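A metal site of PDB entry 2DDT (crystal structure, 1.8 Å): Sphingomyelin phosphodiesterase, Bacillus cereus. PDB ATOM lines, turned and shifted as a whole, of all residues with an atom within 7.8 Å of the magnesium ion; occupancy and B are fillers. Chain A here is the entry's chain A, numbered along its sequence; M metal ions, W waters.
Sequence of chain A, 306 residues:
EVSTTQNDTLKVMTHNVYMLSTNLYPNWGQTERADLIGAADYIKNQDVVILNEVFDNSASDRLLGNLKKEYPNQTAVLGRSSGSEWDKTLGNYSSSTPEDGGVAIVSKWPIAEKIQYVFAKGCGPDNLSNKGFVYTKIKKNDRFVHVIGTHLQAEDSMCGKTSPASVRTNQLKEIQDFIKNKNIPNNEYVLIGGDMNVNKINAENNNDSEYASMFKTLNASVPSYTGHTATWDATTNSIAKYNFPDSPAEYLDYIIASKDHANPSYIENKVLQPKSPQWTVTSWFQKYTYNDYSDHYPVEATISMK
The backbone NH of Gly 102 sits at hydrogen-bond distance from the side-chain carboxylate of Asp 100 (2.8 Å). The guanidinium group (NH2) of Arg 80 lies within hydrogen-bond range of the backbone carbonyl oxygen (O) of Val 54 (3.0 Å). The guanidinium group (NH1) of Arg 80 sits at hydrogen-bond distance from the side-chain hydroxyl (OG) of Ser 60, at 3.0 Å. The side-chain carboxylate (OD1) of Asp 100 is in salt-bridge range of the guanidinium group (NH2) of Arg 80 (3.9 Å). The backbone carbonyl oxygen of Met 19 lies within hydrogen-bond range of the backbone NH of Phe 55, at 3.3 Å. NE of Arg 80 lies close to OD1 of Asn 57. The side-chain hydroxyl (OG) of Ser 60 lies within hydrogen-bond range of the backbone carbonyl oxygen (O) of Asn 57 (2.9 Å). The backbone carbonyl oxygen (O) of Phe 55 lies close to the guanidinium group (NH2) of Arg 80 (3.4 Å).
NH2 of Arg 80 touches the magnesium ion, 3.8 Å away. Five residues have an atom within 4 Å of the magnesium ion: Phe 55, Asn 57, Arg 80, Glu 99 and Asp 100. The nearest printed residue that does not touch the magnesium ion is Asp 56 (4.3 Å).
The magnesium ion is bound by OE1 of Glu 99 (1.9 Å), OD2 of Asp 100 (2.1 Å), O of Phe 55 (2.1 Å), water W2 (2.2 Å), water W1 (2.3 Å) and OD1 of Asn 57 (2.4 Å).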
ATOM      1  N   MET A  19      27.420  13.355 -23.349  1.00  0.00           N
ATOM      2  CA  MET A  19      26.469  12.260 -23.397  1.00  0.00           C
ATOM      3  C   MET A  19      27.170  10.945 -23.128  1.00  0.00           C
ATOM      4  O   MET A  19      27.302  10.088 -24.011  1.00  0.00           O
ATOM      5  CB  MET A  19      25.759  12.219 -24.745  1.00  0.00           C
ATOM      6  CG  MET A  19      24.936  13.469 -24.994  1.00  0.00           C
ATOM      7  SD  MET A  19      23.331  13.111 -25.712  1.00  0.00           S
ATOM      8  CE  MET A  19      22.463  14.656 -25.354  1.00  0.00           C
ATOM      9  N   LEU A  20      27.621  10.796 -21.887  1.00  0.00           N
ATOM     10  CA  LEU A  20      28.316   9.583 -21.475  1.00  0.00           C
ATOM     11  C   LEU A  20      27.399   8.392 -21.649  1.00  0.00           C
ATOM     12  O   LEU A  20      26.174   8.530 -21.691  1.00  0.00           O
ATOM     13  CB  LEU A  20      28.730   9.703 -20.002  1.00  0.00           C
ATOM     14  CG  LEU A  20      29.662  10.878 -19.657  1.00  0.00           C
ATOM     15  CD1 LEU A  20      29.872  10.909 -18.152  1.00  0.00           C
ATOM     16  CD2 LEU A  20      30.987  10.741 -20.393  1.00  0.00           C
ATOM     17  N   SER A  21      27.993   7.211 -21.775  1.00  0.00           N
ATOM     18  CA  SER A  21      27.235   5.981 -21.921  1.00  0.00           C
ATOM     19  C   SER A  21      26.359   5.700 -20.702  1.00  0.00           C
ATOM     20  O   SER A  21      26.837   5.748 -19.559  1.00  0.00           O
ATOM     21  CB  SER A  21      28.179   4.801 -22.142  1.00  0.00           C
ATOM     22  OG  SER A  21      27.473   3.579 -22.036  1.00  0.00           O
ATOM     23  N   VAL A  54      29.157  12.361 -27.944  1.00  0.00           N
ATOM     24  CA  VAL A  54      27.864  11.727 -28.190  1.00  0.00           C
ATOM     25  C   VAL A  54      28.218  10.245 -28.129  1.00  0.00           C
ATOM     26  O   VAL A  54      28.109   9.518 -29.121  1.00  0.00           O
ATOM     27  CB  VAL A  54      27.255  12.099 -29.585  1.00  0.00           C
ATOM     28  CG1 VAL A  54      26.599  13.477 -29.502  1.00  0.00           C
ATOM     29  CG2 VAL A  54      28.343  12.099 -30.656  1.00  0.00           C
ATOM     30  N   PHE A  55      28.680   9.828 -26.949  1.00  0.00           N
ATOM     31  CA  PHE A  55      29.088   8.446 -26.672  1.00  0.00           C
ATOM     32  C   PHE A  55      27.937   7.448 -26.562  1.00  0.00           C
ATOM     33  O   PHE A  55      27.990   6.379 -27.143  1.00  0.00           O
ATOM     34  CB  PHE A  55      29.902   8.375 -25.370  1.00  0.00           C
ATOM     35  CG  PHE A  55      31.229   9.086 -25.427  1.00  0.00           C
ATOM     36  CD1 PHE A  55      31.522  10.109 -24.522  1.00  0.00           C
ATOM     37  CD2 PHE A  55      32.180   8.736 -26.373  1.00  0.00           C
ATOM     38  CE1 PHE A  55      32.757  10.769 -24.559  1.00  0.00           C
ATOM     39  CE2 PHE A  55      33.416   9.386 -26.414  1.00  0.00           C
ATOM     40  CZ  PHE A  55      33.699  10.409 -25.510  1.00  0.00           C
ATOM     41  N   ASP A  56      26.920   7.782 -25.775  1.00  0.00           N
ATOM     42  CA  ASP A  56      25.806   6.870 -25.601  1.00  0.00           C
ATOM     43  C   ASP A  56      25.133   6.647 -26.946  1.00  0.00           C
ATOM     44  O   ASP A  56      24.643   7.585 -27.561  1.00  0.00           O
ATOM     45  CB  ASP A  56      24.779   7.436 -24.615  1.00  0.00           C
ATOM     46  CG  ASP A  56      23.721   6.416 -24.250  1.00  0.00           C
ATOM     47  OD1 ASP A  56      24.062   5.458 -23.521  1.00  0.00           O
ATOM     48  OD2 ASP A  56      22.570   6.563 -24.707  1.00  0.00           O
ATOM     49  N   ASN A  57      25.112   5.395 -27.397  1.00  0.00           N
ATOM     50  CA  ASN A  57      24.526   5.061 -28.690  1.00  0.00           C
ATOM     51  C   ASN A  57      23.059   5.435 -28.861  1.00  0.00           C
ATOM     52  O   ASN A  57      22.691   6.076 -29.852  1.00  0.00           O
ATOM     53  CB  ASN A  57      24.743   3.580 -28.978  1.00  0.00           C
ATOM     54  CG  ASN A  57      26.216   3.215 -29.110  1.00  0.00           C
ATOM     55  OD1 ASN A  57      27.093   4.066 -28.915  1.00  0.00           O
ATOM     56  ND2 ASN A  57      26.490   1.962 -29.433  1.00  0.00           N
ATOM     57  N   SER A  58      22.216   5.072 -27.903  1.00  0.00           N
ATOM     58  CA  SER A  58      20.792   5.393 -28.014  1.00  0.00           C
ATOM     59  C   SER A  58      20.496   6.877 -27.935  1.00  0.00           C
ATOM     60  O   SER A  58      19.751   7.418 -28.758  1.00  0.00           O
ATOM     61  CB  SER A  58      19.984   4.662 -26.927  1.00  0.00           C
ATOM     62  OG  SER A  58      20.021   3.266 -27.124  1.00  0.00           O
ATOM     63  N   SER A  60      22.597   9.378 -28.422  1.00  0.00           N
ATOM     64  CA  SER A  60      23.234  10.103 -29.514  1.00  0.00           C
ATOM     65  C   SER A  60      22.392  10.005 -30.784  1.00  0.00           C
ATOM     66  O   SER A  60      22.201  10.977 -31.507  1.00  0.00           O
ATOM     67  CB  SER A  60      24.643   9.580 -29.780  1.00  0.00           C
ATOM     68  OG  SER A  60      24.613   8.231 -30.208  1.00  0.00           O
ATOM     69  N   VAL A  77      28.789   8.282 -36.046  1.00  0.00           N
ATOM     70  CA  VAL A  77      29.599   8.721 -34.918  1.00  0.00           C
ATOM     71  C   VAL A  77      30.968   8.045 -35.014  1.00  0.00           C
ATOM     72  O   VAL A  77      31.059   6.825 -35.149  1.00  0.00           O
ATOM     73  CB  VAL A  77      28.958   8.330 -33.560  1.00  0.00           C
ATOM     74  CG1 VAL A  77      29.900   8.702 -32.421  1.00  0.00           C
ATOM     75  CG2 VAL A  77      27.627   9.047 -33.397  1.00  0.00           C
ATOM     76  N   LEU A  78      32.011   8.856 -34.967  1.00  0.00           N
ATOM     77  CA  LEU A  78      33.388   8.389 -35.037  1.00  0.00           C
ATOM     78  C   LEU A  78      33.640   7.149 -34.180  1.00  0.00           C
ATOM     79  O   LEU A  78      33.260   7.112 -33.027  1.00  0.00           O
ATOM     80  CB  LEU A  78      34.332   9.496 -34.555  1.00  0.00           C
ATOM     81  CG  LEU A  78      35.762   9.110 -34.208  1.00  0.00           C
ATOM     82  CD1 LEU A  78      36.550   8.806 -35.486  1.00  0.00           C
ATOM     83  CD2 LEU A  78      36.413  10.240 -33.416  1.00  0.00           C
ATOM     84  N   GLY A  79      34.299   6.147 -34.769  1.00  0.00           N
ATOM     85  CA  GLY A  79      34.658   4.935 -34.028  1.00  0.00           C
ATOM     86  C   GLY A  79      33.591   3.936 -33.610  1.00  0.00           C
ATOM     87  O   GLY A  79      33.897   2.996 -32.857  1.00  0.00           O
ATOM     88  N   ARG A  80      32.362   4.106 -34.090  1.00  0.00           N
ATOM     89  CA  ARG A  80      31.289   3.194 -33.723  1.00  0.00           C
ATOM     90  C   ARG A  80      31.129   2.069 -34.743  1.00  0.00           C
ATOM     91  O   ARG A  80      30.635   0.980 -34.406  1.00  0.00           O
ATOM     92  CB  ARG A  80      29.972   3.971 -33.598  1.00  0.00           C
ATOM     93  CG  ARG A  80      28.804   3.166 -33.043  1.00  0.00           C
ATOM     94  CD  ARG A  80      27.590   4.064 -32.763  1.00  0.00           C
ATOM     95  NE  ARG A  80      27.865   5.054 -31.732  1.00  0.00           N
ATOM     96  CZ  ARG A  80      27.047   6.055 -31.418  1.00  0.00           C
ATOM     97  NH1 ARG A  80      25.886   6.195 -32.067  1.00  0.00           N
ATOM     98  NH2 ARG A  80      27.380   6.908 -30.461  1.00  0.00           N
ATOM     99  N   PRO A  98      35.922  -0.391 -26.029  1.00  0.00           N
ATOM    100  CA  PRO A  98      34.691  -0.324 -25.234  1.00  0.00           C
ATOM    101  C   PRO A  98      33.725   0.788 -25.629  1.00  0.00           C
ATOM    102  O   PRO A  98      32.515   0.646 -25.495  1.00  0.00           O
ATOM    103  CB  PRO A  98      35.202  -0.141 -23.808  1.00  0.00           C
ATOM    104  CG  PRO A  98      36.561  -0.813 -23.838  1.00  0.00           C
ATOM    105  CD  PRO A  98      37.110  -0.328 -25.156  1.00  0.00           C
ATOM    106  N   GLU A  99      34.263   1.904 -26.123  1.00  0.00           N
ATOM    107  CA  GLU A  99      33.411   3.044 -26.480  1.00  0.00           C
ATOM    108  C   GLU A  99      33.815   3.671 -27.811  1.00  0.00           C
ATOM    109  O   GLU A  99      34.923   3.461 -28.300  1.00  0.00           O
ATOM    110  CB  GLU A  99      33.497   4.083 -25.354  1.00  0.00           C
ATOM    111  CG  GLU A  99      32.625   5.309 -25.532  1.00  0.00           C
ATOM    112  CD  GLU A  99      31.173   4.937 -25.740  1.00  0.00           C
ATOM    113  OE1 GLU A  99      30.724   4.952 -26.896  1.00  0.00           O
ATOM    114  OE2 GLU A  99      30.504   4.605 -24.735  1.00  0.00           O
ATOM    115  N   ASP A 100      32.906   4.430 -28.418  1.00  0.00           N
ATOM    116  CA  ASP A 100      33.227   5.095 -29.679  1.00  0.00           C
ATOM    117  C   ASP A 100      33.919   6.411 -29.393  1.00  0.00           C
ATOM    118  O   ASP A 100      34.109   6.783 -28.237  1.00  0.00           O
ATOM    119  CB  ASP A 100      31.963   5.322 -30.534  1.00  0.00           C
ATOM    120  CG  ASP A 100      30.885   6.121 -29.805  1.00  0.00           C
ATOM    121  OD1 ASP A 100      31.136   7.280 -29.440  1.00  0.00           O
ATOM    122  OD2 ASP A 100      29.774   5.586 -29.620  1.00  0.00           O
ATOM    123  N   GLY A 101      34.309   7.121 -30.459  1.00  0.00           N
ATOM    124  CA  GLY A 101      34.995   8.388 -30.317  1.00  0.00           C
ATOM    125  C   GLY A 101      34.099   9.566 -29.948  1.00  0.00           C
ATOM    126  O   GLY A 101      34.605  10.627 -29.569  1.00  0.00           O
ATOM    127  N   GLY A 102      32.789   9.392 -30.072  1.00  0.00           N
ATOM    128  CA  GLY A 102      31.847  10.443 -29.699  1.00  0.00           C
ATOM    129  C   GLY A 102      31.785  11.708 -30.541  1.00  0.00           C
ATOM    130  O   GLY A 102      31.219  12.716 -30.101  1.00  0.00           O
HETATM  131 MG    MG M   1      29.086   4.701 -27.825  1.00  0.00          MG
HETATM  132  O   HOH W   1      28.425   3.772 -25.869  1.00  0.00           O
HETATM  133  O   HOH W   2      29.721   2.638 -28.308  1.00  0.00           O
